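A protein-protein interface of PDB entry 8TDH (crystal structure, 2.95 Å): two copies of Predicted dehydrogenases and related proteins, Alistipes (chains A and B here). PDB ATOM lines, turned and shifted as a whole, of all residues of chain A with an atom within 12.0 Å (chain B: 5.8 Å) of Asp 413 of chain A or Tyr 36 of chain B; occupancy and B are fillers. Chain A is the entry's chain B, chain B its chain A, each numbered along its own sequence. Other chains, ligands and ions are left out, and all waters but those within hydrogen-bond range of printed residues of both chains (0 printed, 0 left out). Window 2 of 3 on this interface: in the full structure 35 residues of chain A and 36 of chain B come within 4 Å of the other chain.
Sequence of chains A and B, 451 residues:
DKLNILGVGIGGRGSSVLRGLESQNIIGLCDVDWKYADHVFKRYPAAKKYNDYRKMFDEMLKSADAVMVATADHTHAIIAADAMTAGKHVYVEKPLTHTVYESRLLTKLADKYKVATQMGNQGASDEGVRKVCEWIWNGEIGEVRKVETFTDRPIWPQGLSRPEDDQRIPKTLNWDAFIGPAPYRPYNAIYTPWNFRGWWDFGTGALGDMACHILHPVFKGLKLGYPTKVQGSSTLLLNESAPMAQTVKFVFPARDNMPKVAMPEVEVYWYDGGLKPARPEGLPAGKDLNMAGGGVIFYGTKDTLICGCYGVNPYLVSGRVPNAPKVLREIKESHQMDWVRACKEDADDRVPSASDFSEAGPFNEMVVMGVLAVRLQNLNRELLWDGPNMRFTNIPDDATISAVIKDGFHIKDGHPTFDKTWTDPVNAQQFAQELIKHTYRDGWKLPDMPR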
ATOM      1  N   PHE A 409      -4.858 -21.133 -17.094  1.00  0.00           N
ATOM      2  CA  PHE A 409      -3.474 -20.791 -17.393  1.00  0.00           C
ATOM      3  C   PHE A 409      -3.482 -19.608 -18.359  1.00  0.00           C
ATOM      4  O   PHE A 409      -4.256 -19.618 -19.300  1.00  0.00           O
ATOM      5  CB  PHE A 409      -2.647 -21.938 -17.992  1.00  0.00           C
ATOM      6  CG  PHE A 409      -1.263 -21.490 -18.445  1.00  0.00           C
ATOM      7  CD1 PHE A 409      -1.056 -20.978 -19.701  1.00  0.00           C
ATOM      8  CD2 PHE A 409      -0.185 -21.496 -17.571  1.00  0.00           C
ATOM      9  CE1 PHE A 409       0.190 -20.535 -20.094  1.00  0.00           C
ATOM     10  CE2 PHE A 409       1.056 -21.029 -17.965  1.00  0.00           C
ATOM     11  CZ  PHE A 409       1.233 -20.544 -19.234  1.00  0.00           C
ATOM     12  N   HIS A 410      -2.634 -18.604 -18.131  1.00  0.00           N
ATOM     13  CA  HIS A 410      -2.456 -17.562 -19.125  1.00  0.00           C
ATOM     14  C   HIS A 410      -1.102 -16.907 -18.871  1.00  0.00           C
ATOM     15  O   HIS A 410      -0.651 -16.889 -17.745  1.00  0.00           O
ATOM     16  CB  HIS A 410      -3.646 -16.576 -19.127  1.00  0.00           C
ATOM     17  CG  HIS A 410      -3.637 -15.512 -18.071  1.00  0.00           C
ATOM     18  ND1 HIS A 410      -4.009 -15.717 -16.743  1.00  0.00           N
ATOM     19  CD2 HIS A 410      -3.281 -14.210 -18.167  1.00  0.00           C
ATOM     20  CE1 HIS A 410      -3.870 -14.564 -16.057  1.00  0.00           C
ATOM     21  NE2 HIS A 410      -3.426 -13.624 -16.896  1.00  0.00           N
ATOM     22  N   ILE A 411      -0.463 -16.359 -19.905  1.00  0.00           N
ATOM     23  CA  ILE A 411       0.747 -15.581 -19.717  1.00  0.00           C
ATOM     24  C   ILE A 411       0.422 -14.128 -19.982  1.00  0.00           C
ATOM     25  O   ILE A 411      -0.459 -13.821 -20.758  1.00  0.00           O
ATOM     26  CB  ILE A 411       1.871 -16.068 -20.644  1.00  0.00           C
ATOM     27  CG1 ILE A 411       2.042 -17.549 -20.594  1.00  0.00           C
ATOM     28  CG2 ILE A 411       3.199 -15.371 -20.349  1.00  0.00           C
ATOM     29  CD1 ILE A 411       2.943 -18.051 -21.704  1.00  0.00           C
ATOM     30  N   LYS A 412       1.171 -13.238 -19.353  1.00  0.00           N
ATOM     31  CA  LYS A 412       0.782 -11.846 -19.250  1.00  0.00           C
ATOM     32  C   LYS A 412       2.052 -10.998 -19.274  1.00  0.00           C
ATOM     33  O   LYS A 412       2.656 -10.761 -18.219  1.00  0.00           O
ATOM     34  CB  LYS A 412      -0.049 -11.836 -17.963  1.00  0.00           C
ATOM     35  CG  LYS A 412      -0.767 -10.554 -17.621  1.00  0.00           C
ATOM     36  CD  LYS A 412       0.057  -9.351 -17.158  1.00  0.00           C
ATOM     37  CE  LYS A 412       0.255  -8.278 -18.247  1.00  0.00           C
ATOM     38  NZ  LYS A 412      -0.897  -8.003 -19.146  1.00  0.00           N
ATOM     39  N   ASP A 413       2.444 -10.561 -20.486  1.00  0.00           N
ATOM     40  CA  ASP A 413       3.692  -9.840 -20.717  1.00  0.00           C
ATOM     41  C   ASP A 413       4.858 -10.705 -20.256  1.00  0.00           C
ATOM     42  O   ASP A 413       5.799 -10.204 -19.642  1.00  0.00           O
ATOM     43  CB  ASP A 413       3.776  -8.475 -20.038  1.00  0.00           C
ATOM     44  CG  ASP A 413       3.469  -7.239 -20.888  1.00  0.00           C
ATOM     45  OD1 ASP A 413       3.504  -7.349 -22.153  1.00  0.00           O
ATOM     46  OD2 ASP A 413       3.233  -6.156 -20.269  1.00  0.00           O
ATOM     47  N   GLY A 414       4.767 -12.009 -20.540  1.00  0.00           N
ATOM     48  CA  GLY A 414       5.878 -12.909 -20.306  1.00  0.00           C
ATOM     49  C   GLY A 414       5.819 -13.644 -18.972  1.00  0.00           C
ATOM     50  O   GLY A 414       6.430 -14.706 -18.872  1.00  0.00           O
ATOM     51  N   HIS A 415       5.203 -13.070 -17.922  1.00  0.00           N
ATOM     52  CA  HIS A 415       5.164 -13.737 -16.623  1.00  0.00           C
ATOM     53  C   HIS A 415       3.914 -14.617 -16.562  1.00  0.00           C
ATOM     54  O   HIS A 415       2.837 -14.131 -16.898  1.00  0.00           O
ATOM     55  CB  HIS A 415       5.250 -12.733 -15.467  1.00  0.00           C
ATOM     56  CG  HIS A 415       6.281 -11.637 -15.572  1.00  0.00           C
ATOM     57  ND1 HIS A 415       7.631 -11.900 -15.450  1.00  0.00           N
ATOM     58  CD2 HIS A 415       6.187 -10.296 -15.750  1.00  0.00           C
ATOM     59  CE1 HIS A 415       8.339 -10.760 -15.559  1.00  0.00           C
ATOM     60  NE2 HIS A 415       7.481  -9.773 -15.738  1.00  0.00           N
ATOM     61  N   PRO A 416       4.036 -15.957 -16.324  1.00  0.00           N
ATOM     62  CA  PRO A 416       2.898 -16.878 -16.396  1.00  0.00           C
ATOM     63  C   PRO A 416       2.141 -17.043 -15.080  1.00  0.00           C
ATOM     64  O   PRO A 416       2.647 -16.722 -14.020  1.00  0.00           O
ATOM     65  CB  PRO A 416       3.527 -18.169 -16.833  1.00  0.00           C
ATOM     66  CG  PRO A 416       4.889 -18.136 -16.182  1.00  0.00           C
ATOM     67  CD  PRO A 416       5.302 -16.673 -16.076  1.00  0.00           C
ATOM     68  N   THR A 417       0.922 -17.564 -15.163  1.00  0.00           N
ATOM     69  CA  THR A 417      -0.018 -17.551 -14.068  1.00  0.00           C
ATOM     70  C   THR A 417      -0.737 -18.874 -14.103  1.00  0.00           C
ATOM     71  O   THR A 417      -1.291 -19.192 -15.145  1.00  0.00           O
ATOM     72  CB  THR A 417      -1.047 -16.434 -14.274  1.00  0.00           C
ATOM     73  OG1 THR A 417      -0.332 -15.249 -14.627  1.00  0.00           O
ATOM     74  CG2 THR A 417      -1.959 -16.208 -13.076  1.00  0.00           C
ATOM     75  N   PHE A 418      -0.763 -19.606 -12.981  1.00  0.00           N
ATOM     76  CA  PHE A 418      -1.248 -20.974 -13.001  1.00  0.00           C
ATOM     77  C   PHE A 418      -2.604 -21.105 -12.332  1.00  0.00           C
ATOM     78  O   PHE A 418      -2.872 -22.073 -11.657  1.00  0.00           O
ATOM     79  CB  PHE A 418      -0.167 -21.841 -12.355  1.00  0.00           C
ATOM     80  CG  PHE A 418       1.143 -21.844 -13.126  1.00  0.00           C
ATOM     81  CD1 PHE A 418       1.263 -22.522 -14.341  1.00  0.00           C
ATOM     82  CD2 PHE A 418       2.229 -21.122 -12.658  1.00  0.00           C
ATOM     83  CE1 PHE A 418       2.433 -22.443 -15.069  1.00  0.00           C
ATOM     84  CE2 PHE A 418       3.394 -21.048 -13.384  1.00  0.00           C
ATOM     85  CZ  PHE A 418       3.496 -21.703 -14.588  1.00  0.00           C
ATOM     86  N   GLY B  11      16.123 -12.968 -17.912  1.00  0.00           N
ATOM     87  CA  GLY B  11      14.815 -12.396 -17.645  1.00  0.00           C
ATOM     88  C   GLY B  11      14.017 -13.240 -16.663  1.00  0.00           C
ATOM     89  O   GLY B  11      13.235 -12.692 -15.888  1.00  0.00           O
ATOM     90  N   GLY B  12      14.219 -14.559 -16.716  1.00  0.00           N
ATOM     91  CA  GLY B  12      13.397 -15.495 -15.971  1.00  0.00           C
ATOM     92  C   GLY B  12      14.198 -16.133 -14.852  1.00  0.00           C
ATOM     93  O   GLY B  12      14.538 -15.482 -13.878  1.00  0.00           O
ATOM     94  N   ASP B  31      20.359 -10.060 -22.942  1.00  0.00           N
ATOM     95  CA  ASP B  31      19.065 -10.647 -23.190  1.00  0.00           C
ATOM     96  C   ASP B  31      18.561 -10.155 -24.534  1.00  0.00           C
ATOM     97  O   ASP B  31      18.986  -9.102 -24.970  1.00  0.00           O
ATOM     98  CB  ASP B  31      18.165 -10.335 -22.022  1.00  0.00           C
ATOM     99  CG  ASP B  31      16.969 -11.230 -21.866  1.00  0.00           C
ATOM    100  OD1 ASP B  31      16.174 -11.292 -22.813  1.00  0.00           O
ATOM    101  OD2 ASP B  31      16.897 -11.868 -20.811  1.00  0.00           O
ATOM    102  N   ASP B  33      15.241  -9.618 -25.108  1.00  0.00           N
ATOM    103  CA  ASP B  33      13.974  -8.937 -24.884  1.00  0.00           C
ATOM    104  C   ASP B  33      14.176  -7.866 -23.820  1.00  0.00           C
ATOM    105  O   ASP B  33      14.114  -8.171 -22.641  1.00  0.00           O
ATOM    106  CB  ASP B  33      12.889  -9.939 -24.514  1.00  0.00           C
ATOM    107  CG  ASP B  33      11.460  -9.423 -24.348  1.00  0.00           C
ATOM    108  OD1 ASP B  33      11.192  -8.168 -24.364  1.00  0.00           O
ATOM    109  OD2 ASP B  33      10.597 -10.295 -24.220  1.00  0.00           O
ATOM    110  N   TRP B  34      14.377  -6.605 -24.231  1.00  0.00           N
ATOM    111  CA  TRP B  34      14.809  -5.582 -23.297  1.00  0.00           C
ATOM    112  C   TRP B  34      13.665  -5.093 -22.431  1.00  0.00           C
ATOM    113  O   TRP B  34      13.934  -4.369 -21.480  1.00  0.00           O
ATOM    114  CB  TRP B  34      15.509  -4.434 -24.017  1.00  0.00           C
ATOM    115  CG  TRP B  34      16.929  -4.798 -24.285  1.00  0.00           C
ATOM    116  CD1 TRP B  34      17.426  -6.064 -24.318  1.00  0.00           C
ATOM    117  CD2 TRP B  34      18.024  -3.935 -24.601  1.00  0.00           C
ATOM    118  NE1 TRP B  34      18.769  -6.046 -24.576  1.00  0.00           N
ATOM    119  CE2 TRP B  34      19.160  -4.749 -24.755  1.00  0.00           C
ATOM    120  CE3 TRP B  34      18.168  -2.568 -24.749  1.00  0.00           C
ATOM    121  CZ2 TRP B  34      20.412  -4.237 -25.051  1.00  0.00           C
ATOM    122  CZ3 TRP B  34      19.401  -2.060 -25.065  1.00  0.00           C
ATOM    123  CH2 TRP B  34      20.502  -2.880 -25.206  1.00  0.00           C
ATOM    124  N   LYS B  35      12.459  -5.585 -22.704  1.00  0.00           N
ATOM    125  CA  LYS B  35      11.290  -5.262 -21.909  1.00  0.00           C
ATOM    126  C   LYS B  35      11.103  -6.259 -20.757  1.00  0.00           C
ATOM    127  O   LYS B  35      11.110  -5.863 -19.583  1.00  0.00           O
ATOM    128  CB  LYS B  35      10.111  -5.163 -22.888  1.00  0.00           C
ATOM    129  CG  LYS B  35       8.701  -5.114 -22.293  1.00  0.00           C
ATOM    130  CD  LYS B  35       7.722  -6.010 -23.069  1.00  0.00           C
ATOM    131  CE  LYS B  35       6.438  -5.348 -23.487  1.00  0.00           C
ATOM    132  NZ  LYS B  35       5.764  -4.732 -22.334  1.00  0.00           N
ATOM    133  N   TYR B  36      10.939  -7.557 -21.094  1.00  0.00           N
ATOM    134  CA  TYR B  36      10.813  -8.623 -20.105  1.00  0.00           C
ATOM    135  C   TYR B  36      11.933  -8.597 -19.080  1.00  0.00           C
ATOM    136  O   TYR B  36      11.719  -8.910 -17.920  1.00  0.00           O
ATOM    137  CB  TYR B  36      10.917  -9.951 -20.835  1.00  0.00           C
ATOM    138  CG  TYR B  36      10.674 -11.174 -19.964  1.00  0.00           C
ATOM    139  CD1 TYR B  36       9.520 -11.289 -19.197  1.00  0.00           C
ATOM    140  CD2 TYR B  36      11.605 -12.219 -19.905  1.00  0.00           C
ATOM    141  CE1 TYR B  36       9.279 -12.430 -18.446  1.00  0.00           C
ATOM    142  CE2 TYR B  36      11.410 -13.332 -19.105  1.00  0.00           C
ATOM    143  CZ  TYR B  36      10.239 -13.438 -18.379  1.00  0.00           C
ATOM    144  OH  TYR B  36      10.020 -14.537 -17.592  1.00  0.00           O
ATOM    145  N   ALA B  37      13.096  -8.172 -19.545  1.00  0.00           N
ATOM    146  CA  ALA B  37      14.350  -8.281 -18.863  1.00  0.00           C
ATOM    147  C   ALA B  37      14.815  -7.005 -18.185  1.00  0.00           C
ATOM    148  O   ALA B  37      15.964  -6.906 -17.740  1.00  0.00           O
ATOM    149  CB  ALA B  37      15.322  -8.637 -19.932  1.00  0.00           C
ATOM    150  N   ASP B  38      13.974  -5.972 -18.224  1.00  0.00           N
ATOM    151  CA  ASP B  38      14.527  -4.666 -17.920  1.00  0.00           C
ATOM    152  C   ASP B  38      14.917  -4.622 -16.452  1.00  0.00           C
ATOM    153  O   ASP B  38      15.984  -4.152 -16.087  1.00  0.00           O
ATOM    154  CB  ASP B  38      13.628  -3.527 -18.320  1.00  0.00           C
ATOM    155  CG  ASP B  38      14.377  -2.196 -18.278  1.00  0.00           C
ATOM    156  OD1 ASP B  38      15.528  -2.160 -18.836  1.00  0.00           O
ATOM    157  OD2 ASP B  38      13.820  -1.193 -17.722  1.00  0.00           O
ATOM    158  N   HIS B  39      14.029  -5.194 -15.637  1.00  0.00           N
ATOM    159  CA  HIS B  39      14.132  -5.172 -14.193  1.00  0.00           C
ATOM    160  C   HIS B  39      15.525  -5.624 -13.792  1.00  0.00           C
ATOM    161  O   HIS B  39      16.138  -4.954 -12.986  1.00  0.00           O
ATOM    162  CB  HIS B  39      12.930  -5.903 -13.580  1.00  0.00           C
ATOM    163  CG  HIS B  39      12.900  -7.377 -13.774  1.00  0.00           C
ATOM    164  ND1 HIS B  39      12.143  -8.026 -14.754  1.00  0.00           N
ATOM    165  CD2 HIS B  39      13.575  -8.343 -13.098  1.00  0.00           C
ATOM    166  CE1 HIS B  39      12.366  -9.356 -14.688  1.00  0.00           C
ATOM    167  NE2 HIS B  39      13.220  -9.569 -13.686  1.00  0.00           N
ATOM    168  N   PRO B 193       8.324 -14.587 -24.078  1.00  0.00           N
ATOM    169  CA  PRO B 193       9.055 -15.351 -23.074  1.00  0.00           C
ATOM    170  C   PRO B 193       8.293 -16.556 -22.534  1.00  0.00           C
ATOM    171  O   PRO B 193       7.053 -16.579 -22.606  1.00  0.00           O
ATOM    172  CB  PRO B 193       9.241 -14.322 -21.949  1.00  0.00           C
ATOM    173  CG  PRO B 193       9.204 -13.023 -22.654  1.00  0.00           C
ATOM    174  CD  PRO B 193       8.034 -13.250 -23.581  1.00  0.00           C
ATOM    175  N   TRP B 194       9.076 -17.511 -22.007  1.00  0.00           N
ATOM    176  CA  TRP B 194       8.621 -18.591 -21.156  1.00  0.00           C
ATOM    177  C   TRP B 194       7.964 -19.735 -21.934  1.00  0.00           C
ATOM    178  O   TRP B 194       8.363 -20.863 -21.752  1.00  0.00           O
ATOM    179  CB  TRP B 194       7.716 -18.079 -20.040  1.00  0.00           C
ATOM    180  CG  TRP B 194       7.567 -19.092 -18.942  1.00  0.00           C
ATOM    181  CD1 TRP B 194       8.372 -19.231 -17.848  1.00  0.00           C
ATOM    182  CD2 TRP B 194       6.575 -20.133 -18.860  1.00  0.00           C
ATOM    183  NE1 TRP B 194       7.932 -20.266 -17.075  1.00  0.00           N
ATOM    184  CE2 TRP B 194       6.835 -20.838 -17.666  1.00  0.00           C
ATOM    185  CE3 TRP B 194       5.508 -20.540 -19.665  1.00  0.00           C
ATOM    186  CZ2 TRP B 194       6.062 -21.926 -17.269  1.00  0.00           C
ATOM    187  CZ3 TRP B 194       4.733 -21.611 -19.261  1.00  0.00           C
ATOM    188  CH2 TRP B 194       5.021 -22.312 -18.086  1.00  0.00           C
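NZ of Lys 35 of chain B lies within salt-bridge range of OD1 of Asp 413 of chain A, 3.5 Å away.
N of Tyr 36 of chain B is in hydrogen-bond range of OD1 of Asp 33 of chain B. The backbone carbonyl oxygen (O) of Tyr 36 of chain B lies within hydrogen-bond range of a ring nitrogen (ND1) of His 39 of chain B. OD1 of Asp 33 of chain B lies close to N of Lys 35 of chain B (3.3 Å).
Phe 409 of chain A touches Trp 194 of chain B (CZ to CZ3, 3.7 Å). O of Asp 413 of chain A touches CD1 of Tyr 36 of chain B (3.9 Å). Tyr 36 of chain B touches Gly 414 of chain A. CA of Gly 414 of chain A touches CD of Pro 193 of chain B, at 3.9 Å. Gly 414 of chain A touches Trp 194 of chain B. ND1 of His 415 of chain A touches CE1 of Tyr 36 of chain B, at 3.5 Å. Pro 416 of chain A touches Trp 194 of chain B (CG to CE2, 3.6 Å). Phe 418 of chain A touches Trp 194 of chain B (CZ to CZ2, 3.7 Å).
Asp 413 of chain A touches just these residues of chain B: Lys 35 (3.5 Å) and Tyr 36 (3.9 Å). Of the printed residues of chain B, Gly 414 of chain A touches Tyr 36 (3.7 Å), Pro 193 (3.9 Å) and Trp 194 (3.8 Å). Of the printed residues of chain B, Phe 418 of chain A touches Trp 194. No residue of chain A comes within 4 Å of Gly 11 of chain B. No residue of chain A comes within 4 Å of Gly 12 of chain B. No residue of chain A comes within 4 Å of Asp 33 of chain B. Trp 34 of chain B touches none of the printed residues of chain A. Lys 35 of chain B touches just one residue of chain A: Asp 413 (3.5 Å). Tyr 36 of chain B touches just these residues of chain A: Asp 413 (3.9 Å), Gly 414 (3.7 Å) and His 415 (3.5 Å). No residue of chain A comes within 4 Å of Ala 37 of chain B. No residue of chain A comes within 4 Å of His 39 of chain B. Printed residues of chain A within 4 Å of Pro 193 of chain B: Gly 414 (3.9 Å). Of the printed residues of chain A, Trp 194 of chain B touches Phe 409, Gly 414, Pro 416 and Phe 418. The nearest printed residue of chain B that does not touch Phe 409 of chain A is Pro 193 of chain B (7.8 Å).
Of the 12 printed residues of chain B, 4 touch a printed residue of chain A. Along chain B the printed residues that touch a printed residue of chain A span positions 35 to 194. Printed residues of chain A that touch a printed residue of chain B: Phe 409, Asp 413, Gly 414, His 415, Pro 416 and Phe 418. Hydrophobic or aromatic side chains of chain A that line the printed part of chain B: Phe 409, His 415, Pro 416 and Phe 418. Among the printed residues, 9 pairs touch across the chains. Among the printed residues, Asp or Glu carboxylates within 4 Å of a Lys or Arg side-chain nitrogen of the other chain: Asp 413 of chain A with Lys 35 of chain B.
No position is printed for both chains.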
